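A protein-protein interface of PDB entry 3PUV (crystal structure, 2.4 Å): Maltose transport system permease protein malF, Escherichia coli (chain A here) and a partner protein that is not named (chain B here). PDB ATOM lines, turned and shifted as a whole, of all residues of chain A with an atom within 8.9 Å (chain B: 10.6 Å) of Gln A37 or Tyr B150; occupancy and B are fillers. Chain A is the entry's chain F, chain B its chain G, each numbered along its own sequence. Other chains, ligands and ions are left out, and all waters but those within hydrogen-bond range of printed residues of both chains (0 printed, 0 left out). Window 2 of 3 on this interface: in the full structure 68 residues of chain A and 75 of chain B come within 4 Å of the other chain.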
ATOM      1  N   TYR A  29     -18.976 -32.150   6.222  1.00  0.00           N
ATOM      2  CA  TYR A  29     -17.849 -31.245   6.428  1.00  0.00           C
ATOM      3  C   TYR A  29     -18.236 -30.180   7.453  1.00  0.00           C
ATOM      4  O   TYR A  29     -17.377 -29.640   8.153  1.00  0.00           O
ATOM      5  CB  TYR A  29     -17.421 -30.592   5.108  1.00  0.00           C
ATOM      6  CG  TYR A  29     -16.153 -29.763   5.196  1.00  0.00           C
ATOM      7  CD1 TYR A  29     -14.895 -30.365   5.128  1.00  0.00           C
ATOM      8  CD2 TYR A  29     -16.212 -28.375   5.337  1.00  0.00           C
ATOM      9  CE1 TYR A  29     -13.727 -29.606   5.208  1.00  0.00           C
ATOM     10  CE2 TYR A  29     -15.050 -27.608   5.416  1.00  0.00           C
ATOM     11  CZ  TYR A  29     -13.813 -28.230   5.351  1.00  0.00           C
ATOM     12  OH  TYR A  29     -12.667 -27.474   5.427  1.00  0.00           O
ATOM     13  N   LEU A  30     -19.534 -29.888   7.527  1.00  0.00           N
ATOM     14  CA  LEU A  30     -20.076 -28.959   8.514  1.00  0.00           C
ATOM     15  C   LEU A  30     -20.746 -29.683   9.684  1.00  0.00           C
ATOM     16  O   LEU A  30     -20.739 -29.178  10.805  1.00  0.00           O
ATOM     17  CB  LEU A  30     -21.059 -27.978   7.863  1.00  0.00           C
ATOM     18  CG  LEU A  30     -20.515 -26.891   6.925  1.00  0.00           C
ATOM     19  CD1 LEU A  30     -21.637 -26.296   6.085  1.00  0.00           C
ATOM     20  CD2 LEU A  30     -19.784 -25.792   7.691  1.00  0.00           C
ATOM     21  N   VAL A  31     -21.314 -30.859   9.420  1.00  0.00           N
ATOM     22  CA  VAL A  31     -22.038 -31.631  10.441  1.00  0.00           C
ATOM     23  C   VAL A  31     -21.098 -32.232  11.495  1.00  0.00           C
ATOM     24  O   VAL A  31     -21.314 -32.051  12.697  1.00  0.00           O
ATOM     25  CB  VAL A  31     -22.931 -32.735   9.813  1.00  0.00           C
ATOM     26  CG1 VAL A  31     -23.620 -33.564  10.893  1.00  0.00           C
ATOM     27  CG2 VAL A  31     -23.969 -32.117   8.889  1.00  0.00           C
ATOM     28  N   VAL A  32     -20.063 -32.937  11.039  1.00  0.00           N
ATOM     29  CA  VAL A  32     -19.048 -33.504  11.935  1.00  0.00           C
ATOM     30  C   VAL A  32     -18.229 -32.376  12.577  1.00  0.00           C
ATOM     31  O   VAL A  32     -17.738 -32.513  13.700  1.00  0.00           O
ATOM     32  CB  VAL A  32     -18.124 -34.519  11.201  1.00  0.00           C
ATOM     33  CG1 VAL A  32     -17.131 -35.161  12.166  1.00  0.00           C
ATOM     34  CG2 VAL A  32     -18.952 -35.599  10.513  1.00  0.00           C
ATOM     35  N   LEU A  33     -18.109 -31.263  11.855  1.00  0.00           N
ATOM     36  CA  LEU A  33     -17.443 -30.062  12.355  1.00  0.00           C
ATOM     37  C   LEU A  33     -18.257 -29.393  13.466  1.00  0.00           C
ATOM     38  O   LEU A  33     -17.688 -28.823  14.397  1.00  0.00           O
ATOM     39  CB  LEU A  33     -17.181 -29.086  11.200  1.00  0.00           C
ATOM     40  CG  LEU A  33     -16.179 -27.925  11.298  1.00  0.00           C
ATOM     41  CD1 LEU A  33     -16.842 -26.651  11.800  1.00  0.00           C
ATOM     42  CD2 LEU A  33     -14.938 -28.259  12.131  1.00  0.00           C
ATOM     43  N   MET A  34     -19.584 -29.462  13.359  1.00  0.00           N
ATOM     44  CA  MET A  34     -20.478 -29.012  14.430  1.00  0.00           C
ATOM     45  C   MET A  34     -20.444 -29.994  15.599  1.00  0.00           C
ATOM     46  O   MET A  34     -20.606 -29.601  16.754  1.00  0.00           O
ATOM     47  CB  MET A  34     -21.915 -28.858  13.923  1.00  0.00           C
ATOM     48  CG  MET A  34     -22.184 -27.579  13.143  1.00  0.00           C
ATOM     49  SD  MET A  34     -23.788 -27.598  12.314  1.00  0.00           S
ATOM     50  CE  MET A  34     -23.705 -26.071  11.378  1.00  0.00           C
ATOM     51  N   TYR A  35     -20.228 -31.270  15.282  1.00  0.00           N
ATOM     52  CA  TYR A  35     -20.133 -32.328  16.284  1.00  0.00           C
ATOM     53  C   TYR A  35     -18.835 -32.235  17.091  1.00  0.00           C
ATOM     54  O   TYR A  35     -18.778 -32.693  18.234  1.00  0.00           O
ATOM     55  CB  TYR A  35     -20.244 -33.700  15.611  1.00  0.00           C
ATOM     56  CG  TYR A  35     -20.570 -34.837  16.557  1.00  0.00           C
ATOM     57  CD1 TYR A  35     -21.892 -35.130  16.895  1.00  0.00           C
ATOM     58  CD2 TYR A  35     -19.559 -35.625  17.106  1.00  0.00           C
ATOM     59  CE1 TYR A  35     -22.198 -36.175  17.762  1.00  0.00           C
ATOM     60  CE2 TYR A  35     -19.853 -36.672  17.975  1.00  0.00           C
ATOM     61  CZ  TYR A  35     -21.174 -36.941  18.298  1.00  0.00           C
ATOM     62  OH  TYR A  35     -21.468 -37.977  19.156  1.00  0.00           O
ATOM     63  N   ALA A  36     -17.808 -31.637  16.488  1.00  0.00           N
ATOM     64  CA  ALA A  36     -16.489 -31.491  17.114  1.00  0.00           C
ATOM     65  C   ALA A  36     -16.512 -30.615  18.368  1.00  0.00           C
ATOM     66  O   ALA A  36     -15.806 -30.901  19.338  1.00  0.00           O
ATOM     67  CB  ALA A  36     -15.476 -30.959  16.107  1.00  0.00           C
ATOM     68  N   GLN A  37     -17.315 -29.554  18.340  1.00  0.00           N
ATOM     69  CA  GLN A  37     -17.508 -28.688  19.506  1.00  0.00           C
ATOM     70  C   GLN A  37     -18.915 -28.832  20.096  1.00  0.00           C
ATOM     71  O   GLN A  37     -19.741 -29.585  19.573  1.00  0.00           O
ATOM     72  CB  GLN A  37     -17.189 -27.218  19.182  1.00  0.00           C
ATOM     73  CG  GLN A  37     -17.825 -26.668  17.906  1.00  0.00           C
ATOM     74  CD  GLN A  37     -16.905 -26.752  16.698  1.00  0.00           C
ATOM     75  OE1 GLN A  37     -16.068 -27.650  16.594  1.00  0.00           O
ATOM     76  NE2 GLN A  37     -17.060 -25.811  15.774  1.00  0.00           N
ATOM     77  N   GLY A  38     -19.173 -28.112  21.187  1.00  0.00           N
ATOM     78  CA  GLY A  38     -20.452 -28.182  21.895  1.00  0.00           C
ATOM     79  C   GLY A  38     -21.622 -27.595  21.126  1.00  0.00           C
ATOM     80  O   GLY A  38     -22.013 -26.447  21.353  1.00  0.00           O
ATOM     81  N   GLU A  39     -22.180 -28.389  20.215  1.00  0.00           N
ATOM     82  CA  GLU A  39     -23.349 -27.984  19.437  1.00  0.00           C
ATOM     83  C   GLU A  39     -24.455 -29.029  19.551  1.00  0.00           C
ATOM     84  O   GLU A  39     -25.501 -28.762  20.143  1.00  0.00           O
ATOM     85  CB  GLU A  39     -22.977 -27.744  17.968  1.00  0.00           C
ATOM     86  CG  GLU A  39     -22.030 -26.569  17.736  1.00  0.00           C
ATOM     87  CD  GLU A  39     -22.682 -25.216  17.978  1.00  0.00           C
ATOM     88  OE1 GLU A  39     -23.868 -25.046  17.619  1.00  0.00           O
ATOM     89  OE2 GLU A  39     -22.001 -24.319  18.522  1.00  0.00           O
ATOM     90  N   TYR A  40     -24.203 -30.210  18.980  1.00  0.00           N
ATOM     91  CA  TYR A  40     -25.101 -31.377  19.050  1.00  0.00           C
ATOM     92  C   TYR A  40     -26.529 -31.107  18.563  1.00  0.00           C
ATOM     93  O   TYR A  40     -26.933 -31.608  17.512  1.00  0.00           O
ATOM     94  CB  TYR A  40     -25.098 -31.995  20.457  1.00  0.00           C
ATOM     95  CG  TYR A  40     -23.722 -32.381  20.955  1.00  0.00           C
ATOM     96  CD1 TYR A  40     -23.010 -31.543  21.814  1.00  0.00           C
ATOM     97  CD2 TYR A  40     -23.129 -33.582  20.566  1.00  0.00           C
ATOM     98  CE1 TYR A  40     -21.743 -31.891  22.274  1.00  0.00           C
ATOM     99  CE2 TYR A  40     -21.863 -33.940  21.019  1.00  0.00           C
ATOM    100  CZ  TYR A  40     -21.178 -33.091  21.872  1.00  0.00           C
ATOM    101  OH  TYR A  40     -19.927 -33.442  22.323  1.00  0.00           O
ATOM    102  N   LEU A  41     -27.280 -30.321  19.336  1.00  0.00           N
ATOM    103  CA  LEU A  41     -28.627 -29.886  18.971  1.00  0.00           C
ATOM    104  C   LEU A  41     -28.632 -29.240  17.588  1.00  0.00           C
ATOM    105  O   LEU A  41     -29.574 -29.421  16.818  1.00  0.00           O
ATOM    106  CB  LEU A  41     -29.165 -28.900  20.020  1.00  0.00           C
ATOM    107  CG  LEU A  41     -30.674 -28.654  20.165  1.00  0.00           C
ATOM    108  CD1 LEU A  41     -30.998 -28.203  21.584  1.00  0.00           C
ATOM    109  CD2 LEU A  41     -31.209 -27.646  19.147  1.00  0.00           C
ATOM    110  N   PHE A  42     -27.569 -28.497  17.284  1.00  0.00           N
ATOM    111  CA  PHE A  42     -27.412 -27.852  15.986  1.00  0.00           C
ATOM    112  C   PHE A  42     -26.909 -28.833  14.927  1.00  0.00           C
ATOM    113  O   PHE A  42     -27.199 -28.672  13.745  1.00  0.00           O
ATOM    114  CB  PHE A  42     -26.462 -26.657  16.090  1.00  0.00           C
ATOM    115  CG  PHE A  42     -26.807 -25.522  15.165  1.00  0.00           C
ATOM    116  CD1 PHE A  42     -26.399 -25.539  13.833  1.00  0.00           C
ATOM    117  CD2 PHE A  42     -27.542 -24.434  15.626  1.00  0.00           C
ATOM    118  CE1 PHE A  42     -26.719 -24.493  12.973  1.00  0.00           C
ATOM    119  CE2 PHE A  42     -27.868 -23.380  14.776  1.00  0.00           C
ATOM    120  CZ  PHE A  42     -27.454 -23.410  13.445  1.00  0.00           C
ATOM    121  N   ALA A  43     -26.158 -29.844  15.362  1.00  0.00           N
ATOM    122  CA  ALA A  43     -25.590 -30.846  14.459  1.00  0.00           C
ATOM    123  C   ALA A  43     -26.619 -31.883  14.010  1.00  0.00           C
ATOM    124  O   ALA A  43     -26.561 -32.378  12.881  1.00  0.00           O
ATOM    125  CB  ALA A  43     -24.398 -31.530  15.111  1.00  0.00           C
ATOM    126  N   THR A  46     -29.410 -29.966  11.685  1.00  0.00           N
ATOM    127  CA  THR A  46     -28.898 -29.650  10.351  1.00  0.00           C
ATOM    128  C   THR A  46     -28.767 -30.904   9.484  1.00  0.00           C
ATOM    129  O   THR A  46     -28.759 -30.819   8.255  1.00  0.00           O
ATOM    130  CB  THR A  46     -27.549 -28.877  10.414  1.00  0.00           C
ATOM    131  OG1 THR A  46     -27.278 -28.274   9.145  1.00  0.00           O
ATOM    132  CG2 THR A  46     -26.390 -29.796  10.793  1.00  0.00           C
ATOM    133  N   ALA B 142     -29.830 -16.568  19.456  1.00  0.00           N
ATOM    134  CA  ALA B 142     -29.139 -17.831  19.707  1.00  0.00           C
ATOM    135  C   ALA B 142     -28.868 -18.608  18.419  1.00  0.00           C
ATOM    136  O   ALA B 142     -27.869 -19.319  18.319  1.00  0.00           O
ATOM    137  CB  ALA B 142     -29.937 -18.683  20.686  1.00  0.00           C
ATOM    138  N   LEU B 143     -29.756 -18.461  17.440  1.00  0.00           N
ATOM    139  CA  LEU B 143     -29.605 -19.127  16.150  1.00  0.00           C
ATOM    140  C   LEU B 143     -28.492 -18.497  15.312  1.00  0.00           C
ATOM    141  O   LEU B 143     -27.585 -19.195  14.856  1.00  0.00           O
ATOM    142  CB  LEU B 143     -30.933 -19.118  15.381  1.00  0.00           C
ATOM    143  CG  LEU B 143     -30.999 -19.862  14.044  1.00  0.00           C
ATOM    144  CD1 LEU B 143     -31.089 -21.364  14.268  1.00  0.00           C
ATOM    145  CD2 LEU B 143     -32.183 -19.376  13.227  1.00  0.00           C
ATOM    146  N   PHE B 144     -28.561 -17.183  15.121  1.00  0.00           N
ATOM    147  CA  PHE B 144     -27.595 -16.470  14.283  1.00  0.00           C
ATOM    148  C   PHE B 144     -26.203 -16.372  14.904  1.00  0.00           C
ATOM    149  O   PHE B 144     -25.206 -16.236  14.190  1.00  0.00           O
ATOM    150  CB  PHE B 144     -28.114 -15.080  13.921  1.00  0.00           C
ATOM    151  CG  PHE B 144     -29.159 -15.088  12.849  1.00  0.00           C
ATOM    152  CD1 PHE B 144     -30.505 -14.980  13.172  1.00  0.00           C
ATOM    153  CD2 PHE B 144     -28.796 -15.208  11.511  1.00  0.00           C
ATOM    154  CE1 PHE B 144     -31.478 -14.989  12.171  1.00  0.00           C
ATOM    155  CE2 PHE B 144     -29.760 -15.219  10.504  1.00  0.00           C
ATOM    156  CZ  PHE B 144     -31.100 -15.108  10.833  1.00  0.00           C
ATOM    157  N   ASP B 145     -26.142 -16.436  16.231  1.00  0.00           N
ATOM    158  CA  ASP B 145     -24.867 -16.473  16.935  1.00  0.00           C
ATOM    159  C   ASP B 145     -24.146 -17.786  16.633  1.00  0.00           C
ATOM    160  O   ASP B 145     -22.932 -17.798  16.409  1.00  0.00           O
ATOM    161  CB  ASP B 145     -25.073 -16.305  18.443  1.00  0.00           C
ATOM    162  CG  ASP B 145     -23.792 -15.966  19.176  1.00  0.00           C
ATOM    163  OD1 ASP B 145     -22.800 -15.578  18.521  1.00  0.00           O
ATOM    164  OD2 ASP B 145     -23.779 -16.080  20.420  1.00  0.00           O
ATOM    165  N   ARG B 146     -24.905 -18.880  16.625  1.00  0.00           N
ATOM    166  CA  ARG B 146     -24.383 -20.196  16.279  1.00  0.00           C
ATOM    167  C   ARG B 146     -24.058 -20.291  14.792  1.00  0.00           C
ATOM    168  O   ARG B 146     -23.061 -20.898  14.407  1.00  0.00           O
ATOM    169  CB  ARG B 146     -25.377 -21.299  16.673  1.00  0.00           C
ATOM    170  CG  ARG B 146     -25.068 -22.015  17.992  1.00  0.00           C
ATOM    171  CD  ARG B 146     -25.571 -21.247  19.209  1.00  0.00           C
ATOM    172  NE  ARG B 146     -25.162 -21.876  20.465  1.00  0.00           N
ATOM    173  CZ  ARG B 146     -25.411 -21.377  21.676  1.00  0.00           C
ATOM    174  NH1 ARG B 146     -26.075 -20.234  21.808  1.00  0.00           N
ATOM    175  NH2 ARG B 146     -24.993 -22.022  22.757  1.00  0.00           N
ATOM    176  N   LEU B 147     -24.904 -19.684  13.964  1.00  0.00           N
ATOM    177  CA  LEU B 147     -24.744 -19.741  12.513  1.00  0.00           C
ATOM    178  C   LEU B 147     -23.511 -18.973  12.041  1.00  0.00           C
ATOM    179  O   LEU B 147     -22.833 -19.392  11.100  1.00  0.00           O
ATOM    180  CB  LEU B 147     -26.002 -19.205  11.822  1.00  0.00           C
ATOM    181  CG  LEU B 147     -26.261 -19.590  10.363  1.00  0.00           C
ATOM    182  CD1 LEU B 147     -26.508 -21.090  10.210  1.00  0.00           C
ATOM    183  CD2 LEU B 147     -27.443 -18.804   9.828  1.00  0.00           C
ATOM    184  N   GLY B 148     -23.225 -17.862  12.718  1.00  0.00           N
ATOM    185  CA  GLY B 148     -22.153 -16.945  12.335  1.00  0.00           C
ATOM    186  C   GLY B 148     -20.767 -17.552  12.225  1.00  0.00           C
ATOM    187  O   GLY B 148     -19.974 -17.139  11.377  1.00  0.00           O
ATOM    188  N   GLU B 149     -20.474 -18.532  13.074  1.00  0.00           N
ATOM    189  CA  GLU B 149     -19.152 -19.159  13.089  1.00  0.00           C
ATOM    190  C   GLU B 149     -18.955 -20.236  12.020  1.00  0.00           C
ATOM    191  O   GLU B 149     -17.861 -20.789  11.887  1.00  0.00           O
ATOM    192  CB  GLU B 149     -18.801 -19.677  14.492  1.00  0.00           C
ATOM    193  CG  GLU B 149     -19.823 -20.607  15.140  1.00  0.00           C
ATOM    194  CD  GLU B 149     -19.536 -20.833  16.620  1.00  0.00           C
ATOM    195  OE1 GLU B 149     -19.679 -19.870  17.409  1.00  0.00           O
ATOM    196  OE2 GLU B 149     -19.165 -21.968  16.997  1.00  0.00           O
ATOM    197  N   TYR B 150     -20.005 -20.522  11.252  1.00  0.00           N
ATOM    198  CA  TYR B 150     -19.909 -21.470  10.141  1.00  0.00           C
ATOM    199  C   TYR B 150     -20.078 -20.762   8.798  1.00  0.00           C
ATOM    200  O   TYR B 150     -19.206 -20.858   7.930  1.00  0.00           O
ATOM    201  CB  TYR B 150     -20.901 -22.627  10.319  1.00  0.00           C
ATOM    202  CG  TYR B 150     -20.744 -23.324  11.653  1.00  0.00           C
ATOM    203  CD1 TYR B 150     -21.642 -23.091  12.693  1.00  0.00           C
ATOM    204  CD2 TYR B 150     -19.677 -24.190  11.888  1.00  0.00           C
ATOM    205  CE1 TYR B 150     -21.493 -23.717  13.930  1.00  0.00           C
ATOM    206  CE2 TYR B 150     -19.517 -24.818  13.120  1.00  0.00           C
ATOM    207  CZ  TYR B 150     -20.427 -24.578  14.135  1.00  0.00           C
ATOM    208  OH  TYR B 150     -20.267 -25.200  15.351  1.00  0.00           O
ATOM    209  N   ILE B 151     -21.191 -20.048   8.636  1.00  0.00           N
ATOM    210  CA  ILE B 151     -21.374 -19.144   7.503  1.00  0.00           C
ATOM    211  C   ILE B 151     -21.390 -17.709   8.038  1.00  0.00           C
ATOM    212  O   ILE B 151     -22.431 -17.232   8.493  1.00  0.00           O
ATOM    213  CB  ILE B 151     -22.677 -19.432   6.699  1.00  0.00           C
ATOM    214  CG1 ILE B 151     -22.885 -20.934   6.472  1.00  0.00           C
ATOM    215  CG2 ILE B 151     -22.671 -18.686   5.362  1.00  0.00           C
ATOM    216  CD1 ILE B 151     -23.931 -21.561   7.381  1.00  0.00           C
ATOM    217  N   PRO B 152     -20.230 -17.020   7.998  1.00  0.00           N
ATOM    218  CA  PRO B 152     -20.117 -15.650   8.518  1.00  0.00           C
ATOM    219  C   PRO B 152     -20.964 -14.639   7.743  1.00  0.00           C
ATOM    220  O   PRO B 152     -21.384 -13.626   8.307  1.00  0.00           O
ATOM    221  CB  PRO B 152     -18.626 -15.327   8.349  1.00  0.00           C
ATOM    222  CG  PRO B 152     -17.952 -16.645   8.172  1.00  0.00           C
ATOM    223  CD  PRO B 152     -18.945 -17.501   7.462  1.00  0.00           C
ATOM    224  N   PHE B 153     -21.214 -14.936   6.470  1.00  0.00           N
ATOM    225  CA  PHE B 153     -21.960 -14.066   5.561  1.00  0.00           C
ATOM    226  C   PHE B 153     -23.408 -13.836   6.009  1.00  0.00           C
ATOM    227  O   PHE B 153     -24.013 -12.814   5.673  1.00  0.00           O
ATOM    228  CB  PHE B 153     -21.915 -14.658   4.144  1.00  0.00           C
ATOM    229  CG  PHE B 153     -22.220 -13.667   3.047  1.00  0.00           C
ATOM    230  CD1 PHE B 153     -21.569 -12.432   2.991  1.00  0.00           C
ATOM    231  CD2 PHE B 153     -23.141 -13.984   2.046  1.00  0.00           C
ATOM    232  CE1 PHE B 153     -21.848 -11.515   1.969  1.00  0.00           C
ATOM    233  CE2 PHE B 153     -23.427 -13.077   1.016  1.00  0.00           C
ATOM    234  CZ  PHE B 153     -22.776 -11.839   0.979  1.00  0.00           C
ATOM    235  N   ILE B 154     -23.953 -14.785   6.768  1.00  0.00           N
ATOM    236  CA  ILE B 154     -25.333 -14.694   7.260  1.00  0.00           C
ATOM    237  C   ILE B 154     -25.433 -14.796   8.790  1.00  0.00           C
ATOM    238  O   ILE B 154     -26.422 -15.299   9.323  1.00  0.00           O
ATOM    239  CB  ILE B 154     -26.281 -15.732   6.567  1.00  0.00           C
ATOM    240  CG1 ILE B 154     -25.733 -17.160   6.704  1.00  0.00           C
ATOM    241  CG2 ILE B 154     -26.529 -15.351   5.101  1.00  0.00           C
ATOM    242  CD1 ILE B 154     -26.664 -18.248   6.189  1.00  0.00           C
ATOM    243  N   GLY B 155     -24.409 -14.311   9.487  1.00  0.00           N
ATOM    244  CA  GLY B 155     -24.399 -14.305  10.951  1.00  0.00           C
ATOM    245  C   GLY B 155     -24.836 -12.969  11.524  1.00  0.00           C
ATOM    246  O   GLY B 155     -25.486 -12.175  10.841  1.00  0.00           O
ATOM    247  N   LEU B 156     -24.483 -12.722  12.784  1.00  0.00           N
ATOM    248  CA  LEU B 156     -24.779 -11.447  13.439  1.00  0.00           C
ATOM    249  C   LEU B 156     -24.012 -10.302  12.783  1.00  0.00           C
ATOM    250  O   LEU B 156     -22.908 -10.499  12.272  1.00  0.00           O
ATOM    251  CB  LEU B 156     -24.443 -11.508  14.931  1.00  0.00           C
ATOM    252  CG  LEU B 156     -25.183 -12.516  15.816  1.00  0.00           C
ATOM    253  CD1 LEU B 156     -24.512 -12.621  17.184  1.00  0.00           C
ATOM    254  CD2 LEU B 156     -26.656 -12.159  15.958  1.00  0.00           C
ATOM    255  N   THR B 158     -24.691  -8.650  10.012  1.00  0.00           N
ATOM    256  CA  THR B 158     -24.621  -8.776   8.556  1.00  0.00           C
ATOM    257  C   THR B 158     -25.985  -8.524   7.931  1.00  0.00           C
ATOM    258  O   THR B 158     -27.016  -8.813   8.544  1.00  0.00           O
ATOM    259  CB  THR B 158     -24.158 -10.185   8.115  1.00  0.00           C
ATOM    260  OG1 THR B 158     -25.130 -11.159   8.514  1.00  0.00           O
ATOM    261  CG2 THR B 158     -22.787 -10.542   8.709  1.00  0.00           C
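OH of Tyr B150 lies within hydrogen-bond range of NE2 of Gln A37 (3.3 Å).
Printed residues of chain A that touch a printed residue of chain B: Leu A33, Met A34, Gln A37, Glu A39 and Phe A42. Hydrophobic or aromatic side chains of chain A within 4 Å of the printed part of chain B: Leu A33, Met A34 and Phe A42. Printed residues of chain B that touch a printed residue of chain A: Leu B143, Arg B146, Glu B149 and Tyr B150. Hydrophobic or aromatic side chains of chain B that line the printed part of chain A: Leu B143 and Tyr B150.
Among the printed residues, merely in contact across the chains: Leu A33 with Tyr B150 (3.5 Å), Met A34 with Tyr B150 (3.6 Å), Glu A39 with Arg B146 (3.3 Å), Glu A39 with Glu B149 (3.99 Å), Glu A39 with Tyr B150 (3.3 Å), Phe A42 with Leu B143 (3.8 Å) and Phe A42 with Arg B146 (3.8 Å).
Leu A33 touches one residue of chain B. Ala A36 touches none of the printed residues of chain B. Printed residues of chain B within 4 Å of Gln A37: Tyr B150. Gly A38 touches none of the printed residues of chain B. Printed residues of chain B within 4 Å of Glu A39: Arg B146, Glu B149 and Tyr B150. Printed residues of chain A within 4 Å of Arg B146: Glu A39 and Phe A42. No residue of chain A comes within 4 Å of Gly B148. Of the printed residues of chain A, Glu B149 touches Glu A39 (3.99 Å). Tyr B150 touches four residues of chain A. No residue of chain A comes within 4 Å of Ile B151. Leu B156 touches none of the printed residues of chain A. The nearest residue of chain A that does not touch Tyr B150 is Leu A30 (4.3 Å). The nearest printed residue of chain A that does not touch Leu B143 is Glu A39 (7.5 Å).
The backbone carbonyl oxygen of Leu A33 lies close to the side-chain amide oxygen of Gln A37.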
